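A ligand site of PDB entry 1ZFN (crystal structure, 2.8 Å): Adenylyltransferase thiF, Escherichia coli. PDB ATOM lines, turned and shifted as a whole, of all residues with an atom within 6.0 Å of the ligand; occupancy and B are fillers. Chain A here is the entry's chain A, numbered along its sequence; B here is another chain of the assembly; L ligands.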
ATOM      1  N   ILE A  36      -7.520  33.287   7.171  1.00  0.00           N
ATOM      2  CA  ILE A  36      -6.389  32.429   7.525  1.00  0.00           C
ATOM      3  C   ILE A  36      -5.803  31.843   6.229  1.00  0.00           C
ATOM      4  O   ILE A  36      -6.439  31.020   5.566  1.00  0.00           O
ATOM      5  CB  ILE A  36      -6.796  31.227   8.446  1.00  0.00           C
ATOM      6  CG1 ILE A  36      -7.825  31.627   9.507  1.00  0.00           C
ATOM      7  CG2 ILE A  36      -5.583  30.731   9.192  1.00  0.00           C
ATOM      8  CD1 ILE A  36      -9.220  31.732   8.973  1.00  0.00           C
ATOM      9  N   GLY A  37      -4.596  32.263   5.872  1.00  0.00           N
ATOM     10  CA  GLY A  37      -3.977  31.743   4.660  1.00  0.00           C
ATOM     11  C   GLY A  37      -3.993  32.761   3.537  1.00  0.00           C
ATOM     12  O   GLY A  37      -5.059  33.221   3.132  1.00  0.00           O
ATOM     13  N   LEU A  38      -2.808  33.108   3.018  1.00  0.00           N
ATOM     14  CA  LEU A  38      -2.739  34.105   1.957  1.00  0.00           C
ATOM     15  C   LEU A  38      -2.062  33.560   0.687  1.00  0.00           C
ATOM     16  O   LEU A  38      -1.123  34.138   0.145  1.00  0.00           O
ATOM     17  CB  LEU A  38      -2.015  35.352   2.466  1.00  0.00           C
ATOM     18  CG  LEU A  38      -2.616  36.003   3.736  1.00  0.00           C
ATOM     19  CD1 LEU A  38      -1.695  37.106   4.239  1.00  0.00           C
ATOM     20  CD2 LEU A  38      -4.008  36.535   3.448  1.00  0.00           C
ATOM     21  N   GLY A  39      -2.575  32.427   0.225  1.00  0.00           N
ATOM     22  CA  GLY A  39      -2.050  31.791  -0.965  1.00  0.00           C
ATOM     23  C   GLY A  39      -2.948  31.991  -2.170  1.00  0.00           C
ATOM     24  O   GLY A  39      -3.329  33.116  -2.491  1.00  0.00           O
ATOM     25  N   GLY A  40      -3.282  30.896  -2.836  1.00  0.00           N
ATOM     26  CA  GLY A  40      -4.101  30.944  -4.027  1.00  0.00           C
ATOM     27  C   GLY A  40      -5.538  31.350  -3.789  1.00  0.00           C
ATOM     28  O   GLY A  40      -6.154  31.973  -4.654  1.00  0.00           O
ATOM     29  N   LEU A  41      -6.081  30.992  -2.638  1.00  0.00           N
ATOM     30  CA  LEU A  41      -7.454  31.350  -2.312  1.00  0.00           C
ATOM     31  C   LEU A  41      -7.497  32.705  -1.600  1.00  0.00           C
ATOM     32  O   LEU A  41      -8.206  33.618  -2.029  1.00  0.00           O
ATOM     33  CB  LEU A  41      -8.077  30.299  -1.396  1.00  0.00           C
ATOM     34  CG  LEU A  41      -8.275  28.869  -1.875  1.00  0.00           C
ATOM     35  CD1 LEU A  41      -8.447  28.005  -0.635  1.00  0.00           C
ATOM     36  CD2 LEU A  41      -9.492  28.742  -2.803  1.00  0.00           C
ATOM     37  N   ALA A  60      -3.763  36.342   8.202  1.00  0.00           N
ATOM     38  CA  ALA A  60      -2.847  35.433   8.889  1.00  0.00           C
ATOM     39  C   ALA A  60      -2.124  34.466   7.955  1.00  0.00           C
ATOM     40  O   ALA A  60      -2.749  33.742   7.180  1.00  0.00           O
ATOM     41  CB  ALA A  60      -3.602  34.634   9.957  1.00  0.00           C
ATOM     42  N   ASP A  61      -0.805  34.467   8.030  1.00  0.00           N
ATOM     43  CA  ASP A  61      -0.013  33.562   7.223  1.00  0.00           C
ATOM     44  C   ASP A  61       1.416  33.520   7.717  1.00  0.00           C
ATOM     45  O   ASP A  61       2.064  34.560   7.906  1.00  0.00           O
ATOM     46  CB  ASP A  61      -0.041  33.969   5.751  1.00  0.00           C
ATOM     47  CG  ASP A  61       0.382  32.823   4.831  1.00  0.00           C
ATOM     48  OD1 ASP A  61       1.518  32.328   4.975  1.00  0.00           O
ATOM     49  OD2 ASP A  61      -0.422  32.429   3.967  1.00  0.00           O
ATOM     50  N   ASP A  62       1.911  32.296   7.912  1.00  0.00           N
ATOM     51  CA  ASP A  62       3.250  32.062   8.411  1.00  0.00           C
ATOM     52  C   ASP A  62       4.314  31.839   7.333  1.00  0.00           C
ATOM     53  O   ASP A  62       5.502  31.773   7.641  1.00  0.00           O
ATOM     54  CB  ASP A  62       3.222  30.847   9.342  1.00  0.00           C
ATOM     55  CG  ASP A  62       4.394  30.819  10.288  1.00  0.00           C
ATOM     56  OD1 ASP A  62       4.460  29.872  11.099  1.00  0.00           O
ATOM     57  OD2 ASP A  62       5.245  31.727  10.232  1.00  0.00           O
ATOM     58  N   ASP A  63       3.902  31.766   6.071  1.00  0.00           N
ATOM     59  CA  ASP A  63       4.834  31.534   4.975  1.00  0.00           C
ATOM     60  C   ASP A  63       5.424  32.811   4.365  1.00  0.00           C
ATOM     61  O   ASP A  63       4.981  33.927   4.648  1.00  0.00           O
ATOM     62  CB  ASP A  63       4.122  30.737   3.873  1.00  0.00           C
ATOM     63  CG  ASP A  63       5.047  29.774   3.138  1.00  0.00           C
ATOM     64  OD1 ASP A  63       6.256  30.073   3.018  1.00  0.00           O
ATOM     65  OD2 ASP A  63       4.554  28.730   2.664  1.00  0.00           O
ATOM     66  N   HIS A  66       7.283  32.768  -2.294  1.00  0.00           N
ATOM     67  CA  HIS A  66       8.188  31.962  -3.102  1.00  0.00           C
ATOM     68  C   HIS A  66       7.866  32.163  -4.567  1.00  0.00           C
ATOM     69  O   HIS A  66       6.735  32.491  -4.918  1.00  0.00           O
ATOM     70  CB  HIS A  66       8.049  30.489  -2.750  1.00  0.00           C
ATOM     71  CG  HIS A  66       8.166  30.215  -1.283  1.00  0.00           C
ATOM     72  ND1 HIS A  66       9.306  30.502  -0.570  1.00  0.00           N
ATOM     73  CD2 HIS A  66       7.276  29.711  -0.392  1.00  0.00           C
ATOM     74  CE1 HIS A  66       9.116  30.179   0.700  1.00  0.00           C
ATOM     75  NE2 HIS A  66       7.891  29.694   0.835  1.00  0.00           N
ATOM     76  N   SER A  68       7.383  30.118  -7.086  1.00  0.00           N
ATOM     77  CA  SER A  68       6.313  29.294  -7.660  1.00  0.00           C
ATOM     78  C   SER A  68       4.920  29.832  -7.353  1.00  0.00           C
ATOM     79  O   SER A  68       3.939  29.439  -7.993  1.00  0.00           O
ATOM     80  CB  SER A  68       6.415  27.841  -7.165  1.00  0.00           C
ATOM     81  OG  SER A  68       6.063  27.714  -5.808  1.00  0.00           O
ATOM     82  N   ASN A  69       4.837  30.726  -6.368  1.00  0.00           N
ATOM     83  CA  ASN A  69       3.560  31.296  -5.978  1.00  0.00           C
ATOM     84  C   ASN A  69       3.049  32.250  -7.050  1.00  0.00           C
ATOM     85  O   ASN A  69       1.854  32.282  -7.351  1.00  0.00           O
ATOM     86  CB  ASN A  69       3.695  32.048  -4.651  1.00  0.00           C
ATOM     87  CG  ASN A  69       4.064  31.147  -3.496  1.00  0.00           C
ATOM     88  OD1 ASN A  69       3.687  29.974  -3.448  1.00  0.00           O
ATOM     89  ND2 ASN A  69       4.789  31.693  -2.535  1.00  0.00           N
ATOM     90  N   ARG A  72      -0.221  32.210  -9.390  1.00  0.00           N
ATOM     91  CA  ARG A  72      -1.637  32.290  -9.029  1.00  0.00           C
ATOM     92  C   ARG A  72      -1.971  33.158  -7.811  1.00  0.00           C
ATOM     93  O   ARG A  72      -3.151  33.463  -7.552  1.00  0.00           O
ATOM     94  CB  ARG A  72      -2.156  30.873  -8.793  1.00  0.00           C
ATOM     95  CG  ARG A  72      -1.776  30.317  -7.437  1.00  0.00           C
ATOM     96  CD  ARG A  72      -1.902  28.822  -7.387  1.00  0.00           C
ATOM     97  NE  ARG A  72      -0.617  28.255  -7.024  1.00  0.00           N
ATOM     98  CZ  ARG A  72      -0.330  27.726  -5.844  1.00  0.00           C
ATOM     99  NH1 ARG A  72      -1.273  27.681  -4.892  1.00  0.00           N
ATOM    100  NH2 ARG A  72       0.903  27.283  -5.594  1.00  0.00           N
ATOM    101  N   GLN A  73      -0.958  33.532  -7.043  1.00  0.00           N
ATOM    102  CA  GLN A  73      -1.191  34.362  -5.881  1.00  0.00           C
ATOM    103  C   GLN A  73      -0.986  35.796  -6.346  1.00  0.00           C
ATOM    104  O   GLN A  73       0.022  36.444  -6.054  1.00  0.00           O
ATOM    105  CB  GLN A  73      -0.212  33.967  -4.776  1.00  0.00           C
ATOM    106  CG  GLN A  73      -0.058  32.465  -4.673  1.00  0.00           C
ATOM    107  CD  GLN A  73       0.464  31.983  -3.343  1.00  0.00           C
ATOM    108  OE1 GLN A  73       1.245  32.666  -2.689  1.00  0.00           O
ATOM    109  NE2 GLN A  73       0.054  30.785  -2.947  1.00  0.00           N
ATOM    110  N   LYS A  85       4.596  36.725   3.585  1.00  0.00           N
ATOM    111  CA  LYS A  85       3.307  36.894   2.947  1.00  0.00           C
ATOM    112  C   LYS A  85       2.357  37.877   3.615  1.00  0.00           C
ATOM    113  O   LYS A  85       1.845  38.779   2.961  1.00  0.00           O
ATOM    114  CB  LYS A  85       2.624  35.528   2.806  1.00  0.00           C
ATOM    115  CG  LYS A  85       3.268  34.642   1.757  1.00  0.00           C
ATOM    116  CD  LYS A  85       2.455  33.361   1.530  1.00  0.00           C
ATOM    117  CE  LYS A  85       2.965  32.596   0.313  1.00  0.00           C
ATOM    118  NZ  LYS A  85       2.056  31.485  -0.127  1.00  0.00           N
ATOM    119  N   GLN A 107       2.015  34.259  11.456  1.00  0.00           N
ATOM    120  CA  GLN A 107       2.047  33.029  12.237  1.00  0.00           C
ATOM    121  C   GLN A 107       1.073  31.960  11.733  1.00  0.00           C
ATOM    122  O   GLN A 107       0.341  32.174  10.770  1.00  0.00           O
ATOM    123  CB  GLN A 107       1.722  33.342  13.701  1.00  0.00           C
ATOM    124  CG  GLN A 107       0.628  34.396  13.879  1.00  0.00           C
ATOM    125  CD  GLN A 107       0.069  34.436  15.288  1.00  0.00           C
ATOM    126  OE1 GLN A 107       0.776  34.219  16.270  1.00  0.00           O
ATOM    127  NE2 GLN A 107      -1.224  34.742  15.396  1.00  0.00           N
ATOM    128  N   ARG A 108       1.064  30.800  12.387  1.00  0.00           N
ATOM    129  CA  ARG A 108       0.136  29.747  12.026  1.00  0.00           C
ATOM    130  C   ARG A 108      -0.911  29.671  13.124  1.00  0.00           C
ATOM    131  O   ARG A 108      -0.634  29.175  14.229  1.00  0.00           O
ATOM    132  CB  ARG A 108       0.846  28.394  11.917  1.00  0.00           C
ATOM    133  CG  ARG A 108       1.568  28.175  10.608  1.00  0.00           C
ATOM    134  CD  ARG A 108       2.088  26.759  10.560  1.00  0.00           C
ATOM    135  NE  ARG A 108       2.873  26.486   9.362  1.00  0.00           N
ATOM    136  CZ  ARG A 108       3.551  25.360   9.162  1.00  0.00           C
ATOM    137  NH1 ARG A 108       3.547  24.405  10.089  1.00  0.00           N
ATOM    138  NH2 ARG A 108       4.249  25.196   8.049  1.00  0.00           N
ATOM    139  N   LEU A 109      -2.107  30.163  12.831  1.00  0.00           N
ATOM    140  CA  LEU A 109      -3.158  30.163  13.836  1.00  0.00           C
ATOM    141  C   LEU A 109      -3.525  28.778  14.353  1.00  0.00           C
ATOM    142  O   LEU A 109      -3.914  27.894  13.581  1.00  0.00           O
ATOM    143  CB  LEU A 109      -4.407  30.868  13.290  1.00  0.00           C
ATOM    144  CG  LEU A 109      -4.227  32.371  13.054  1.00  0.00           C
ATOM    145  CD1 LEU A 109      -5.568  33.026  12.794  1.00  0.00           C
ATOM    146  CD2 LEU A 109      -3.572  32.983  14.275  1.00  0.00           C
ATOM    147  N   THR A 110      -3.404  28.606  15.661  1.00  0.00           N
ATOM    148  CA  THR A 110      -3.708  27.345  16.325  1.00  0.00           C
ATOM    149  C   THR A 110      -4.206  27.677  17.721  1.00  0.00           C
ATOM    150  O   THR A 110      -4.690  28.780  17.964  1.00  0.00           O
ATOM    151  CB  THR A 110      -2.466  26.467  16.501  1.00  0.00           C
ATOM    152  OG1 THR A 110      -1.577  26.677  15.397  1.00  0.00           O
ATOM    153  CG2 THR A 110      -2.850  24.987  16.575  1.00  0.00           C
ATOM    154  N   CYS A 127      -8.641  29.754   4.246  1.00  0.00           N
ATOM    155  CA  CYS A 127      -7.952  29.836   2.959  1.00  0.00           C
ATOM    156  C   CYS A 127      -6.682  29.031   3.025  1.00  0.00           C
ATOM    157  O   CYS A 127      -5.724  29.264   2.279  1.00  0.00           O
ATOM    158  CB  CYS A 127      -7.650  31.282   2.608  1.00  0.00           C
ATOM    159  SG  CYS A 127      -9.129  32.145   2.075  1.00  0.00           S
ATOM    160  N   THR A 128      -6.675  28.085   3.952  1.00  0.00           N
ATOM    161  CA  THR A 128      -5.554  27.190   4.129  1.00  0.00           C
ATOM    162  C   THR A 128      -5.899  25.925   3.364  1.00  0.00           C
ATOM    163  O   THR A 128      -7.046  25.488   3.352  1.00  0.00           O
ATOM    164  CB  THR A 128      -5.386  26.791   5.598  1.00  0.00           C
ATOM    165  OG1 THR A 128      -6.576  26.127   6.041  1.00  0.00           O
ATOM    166  CG2 THR A 128      -5.163  28.019   6.463  1.00  0.00           C
ATOM    167  N   ASP A 129      -4.916  25.355   2.686  1.00  0.00           N
ATOM    168  CA  ASP A 129      -5.167  24.112   1.996  1.00  0.00           C
ATOM    169  C   ASP A 129      -4.433  23.137   2.901  1.00  0.00           C
ATOM    170  O   ASP A 129      -3.282  22.783   2.665  1.00  0.00           O
ATOM    171  CB  ASP A 129      -4.579  24.145   0.588  1.00  0.00           C
ATOM    172  CG  ASP A 129      -5.481  24.889  -0.394  1.00  0.00           C
ATOM    173  OD1 ASP A 129      -6.532  24.328  -0.767  1.00  0.00           O
ATOM    174  OD2 ASP A 129      -5.137  26.024  -0.777  1.00  0.00           O
ATOM    175  N   ASN A 130      -5.110  22.758   3.971  1.00  0.00           N
ATOM    176  CA  ASN A 130      -4.551  21.870   4.975  1.00  0.00           C
ATOM    177  C   ASN A 130      -5.702  21.337   5.826  1.00  0.00           C
ATOM    178  O   ASN A 130      -6.245  22.057   6.652  1.00  0.00           O
ATOM    179  CB  ASN A 130      -3.557  22.667   5.816  1.00  0.00           C
ATOM    180  CG  ASN A 130      -3.021  21.881   6.983  1.00  0.00           C
ATOM    181  OD1 ASN A 130      -3.782  21.381   7.819  1.00  0.00           O
ATOM    182  ND2 ASN A 130      -1.697  21.775   7.072  1.00  0.00           N
ATOM    183  N   THR A 133      -5.520  22.158   9.857  1.00  0.00           N
ATOM    184  CA  THR A 133      -5.862  23.539  10.177  1.00  0.00           C
ATOM    185  C   THR A 133      -7.351  23.740   9.965  1.00  0.00           C
ATOM    186  O   THR A 133      -8.052  24.290  10.802  1.00  0.00           O
ATOM    187  CB  THR A 133      -5.125  24.512   9.254  1.00  0.00           C
ATOM    188  OG1 THR A 133      -3.722  24.181   9.213  1.00  0.00           O
ATOM    189  CG2 THR A 133      -5.303  25.934   9.743  1.00  0.00           C
ATOM    190  N   GLU A 136      -9.656  22.384  12.737  1.00  0.00           N
ATOM    191  CA  GLU A 136      -9.671  23.091  14.001  1.00  0.00           C
ATOM    192  C   GLU A 136     -10.262  24.490  13.858  1.00  0.00           C
ATOM    193  O   GLU A 136     -10.699  25.096  14.832  1.00  0.00           O
ATOM    194  CB  GLU A 136      -8.268  23.150  14.628  1.00  0.00           C
ATOM    195  CG  GLU A 136      -7.425  24.344  14.277  1.00  0.00           C
ATOM    196  CD  GLU A 136      -6.207  24.438  15.191  1.00  0.00           C
ATOM    197  OE1 GLU A 136      -6.390  24.490  16.426  1.00  0.00           O
ATOM    198  OE2 GLU A 136      -5.061  24.479  14.670  1.00  0.00           O
ATOM    199  N   VAL A 196      -8.224  28.050  -8.798  1.00  0.00           N
ATOM    200  CA  VAL A 196      -8.209  28.403  -7.388  1.00  0.00           C
ATOM    201  C   VAL A 196      -8.645  29.855  -7.240  1.00  0.00           C
ATOM    202  O   VAL A 196      -9.224  30.234  -6.223  1.00  0.00           O
ATOM    203  CB  VAL A 196      -6.821  28.196  -6.725  1.00  0.00           C
ATOM    204  CG1 VAL A 196      -5.783  29.149  -7.280  1.00  0.00           C
ATOM    205  CG2 VAL A 196      -6.962  28.353  -5.231  1.00  0.00           C
ATOM    206  N   ARG B  13       3.552  24.555 -10.648  1.00  0.00           N
ATOM    207  CA  ARG B  13       2.219  24.036 -10.329  1.00  0.00           C
ATOM    208  C   ARG B  13       1.323  23.765 -11.533  1.00  0.00           C
ATOM    209  O   ARG B  13       0.201  23.278 -11.367  1.00  0.00           O
ATOM    210  CB  ARG B  13       1.517  24.946  -9.333  1.00  0.00           C
ATOM    211  CG  ARG B  13       1.898  24.684  -7.873  1.00  0.00           C
ATOM    212  CD  ARG B  13       3.389  24.800  -7.616  1.00  0.00           C
ATOM    213  NE  ARG B  13       3.713  24.498  -6.222  1.00  0.00           N
ATOM    214  CZ  ARG B  13       4.961  24.366  -5.754  1.00  0.00           C
ATOM    215  NH1 ARG B  13       6.000  24.527  -6.587  1.00  0.00           N
ATOM    216  NH2 ARG B  13       5.175  24.085  -4.470  1.00  0.00           N
HETATM  217  P1  LIG L   1       2.149  25.566  -2.778  1.00  0.00           P
HETATM  218  O1  LIG L   1       2.794  24.860  -1.719  1.00  0.00           O
HETATM  219  O2  LIG L   1       2.976  26.199  -3.956  1.00  0.00           O
HETATM  220  O3  LIG L   1       1.103  24.545  -3.129  1.00  0.00           O
HETATM  221  P2  LIG L   1       1.093  27.374  -0.803  1.00  0.00           P
HETATM  222  O4  LIG L   1       0.645  26.488   0.305  1.00  0.00           O
HETATM  223  O5  LIG L   1       1.524  28.749  -0.414  1.00  0.00           O
HETATM  224  O6  LIG L   1       1.369  26.839  -2.254  1.00  0.00           O
HETATM  225  P3  LIG L   1      -1.787  27.589  -1.090  1.00  0.00           P
HETATM  226  O7  LIG L   1      -2.571  28.536  -1.760  1.00  0.00           O
HETATM  227  O8  LIG L   1      -2.275  26.138  -0.981  1.00  0.00           O
HETATM  228  O9  LIG L   1      -0.267  27.924  -1.526  1.00  0.00           O
HETATM  229  O10 LIG L   1      -1.540  28.096   0.375  1.00  0.00           O
HETATM  230  C1  LIG L   1      -2.444  28.659   1.200  1.00  0.00           C
HETATM  231  C2  LIG L   1      -1.777  29.447   2.356  1.00  0.00           C
HETATM  232  O11 LIG L   1      -2.154  29.250   3.676  1.00  0.00           O
HETATM  233  C3  LIG L   1      -0.174  29.463   2.346  1.00  0.00           C
HETATM  234  O12 LIG L   1       0.406  30.695   2.011  1.00  0.00           O
HETATM  235  C4  LIG L   1       0.031  28.756   3.655  1.00  0.00           C
HETATM  236  O13 LIG L   1       1.281  29.170   4.117  1.00  0.00           O
HETATM  237  C5  LIG L   1      -1.058  29.209   4.524  1.00  0.00           C
HETATM  238  N1  LIG L   1      -1.414  28.374   5.677  1.00  0.00           N
HETATM  239  C6  LIG L   1      -1.586  27.021   5.751  1.00  0.00           C
HETATM  240  N2  LIG L   1      -1.945  26.666   7.003  1.00  0.00           N
HETATM  241  C7  LIG L   1      -1.999  27.801   7.746  1.00  0.00           C
HETATM  242  C8  LIG L   1      -2.307  28.047   9.112  1.00  0.00           C
HETATM  243  N3  LIG L   1      -2.675  27.138  10.002  1.00  0.00           N
HETATM  244  N4  LIG L   1      -2.267  29.362   9.559  1.00  0.00           N
HETATM  245  C9  LIG L   1      -1.939  30.429   8.719  1.00  0.00           C
HETATM  246  N5  LIG L   1      -1.648  30.164   7.385  1.00  0.00           N
HETATM  247  C10 LIG L   1      -1.660  28.878   6.906  1.00  0.00           C
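The backbone NH of Gly 40 sits at hydrogen-bond distance from an oxygen (O7) of the ligand (2.7 Å). The side-chain carboxylate (OD2) of Asp 61 lies within hydrogen-bond range of an oxygen (O12) of the ligand, 2.7 Å away. An oxygen (O5) of the ligand is in salt-bridge range of the side-chain amino group (NZ) of Lys 85, 2.8 Å away. O2 of the ligand is in salt-bridge range of NH2 of Arg 72 (2.9 Å). The side-chain carboxylate (OD2) of Asp 129 sits close to an oxygen (O8) of the ligand (2.9 Å). OG1 of Thr 133 lies close to N3 of the ligand (3.2 Å). The guanidinium group (NE) of Arg 13 of chain B lies within salt-bridge range of an oxygen (O2) of the ligand, 2.9 Å away. The side-chain amide nitrogen (NE2) of Gln 73 sits at hydrogen-bond distance from an oxygen (O9) of the ligand (3.2 Å). The backbone NH (N) of Leu 109 is in hydrogen-bond range of a nitrogen (N4) of the ligand (3.4 Å).
The side-chain amide nitrogen (NE2) of Gln 73 sits close to the backbone NH (N) of Gly 40. The side-chain carboxylate (OD1) of Asp 61 is in hydrogen-bond range of the backbone NH (N) of Asp 63, at 2.7 Å. NZ of Lys 85 sits at hydrogen-bond distance from OE1 of Gln 73 (2.9 Å). OD1 of Asn 130 is in hydrogen-bond range of N of Thr 133 (2.8 Å). The guanidinium group (NH1) of Arg 13 of chain B lies within hydrogen-bond range of the side-chain hydroxyl (OG) of Ser 68 (3.3 Å). The backbone carbonyl oxygen of Ala 60 lies within hydrogen-bond range of the backbone NH of Gly 37, at 2.7 Å. N of Cys 127 sits at hydrogen-bond distance from O of Ile 36 (2.9 Å). N of Asp 62 is in hydrogen-bond range of O of Gln 107 (3.3 Å).
Residues that only touch the ligand: Gly 37 (3.2 Å), Asp 63 (3.3 Å), Gly 39 (3.4 Å), Thr 128 (3.4 Å), Arg 108 (3.5 Å), Cys 127 (3.5 Å), Gln 107 (3.5 Å), Ile 36 (3.6 Å), Ala 60 (3.7 Å), Leu 38 (3.9 Å), Asn 69 (3.9 Å) and Ser 68 (3.9 Å). Hydrophobic or aromatic side chains that line the ligand: Ile 36.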
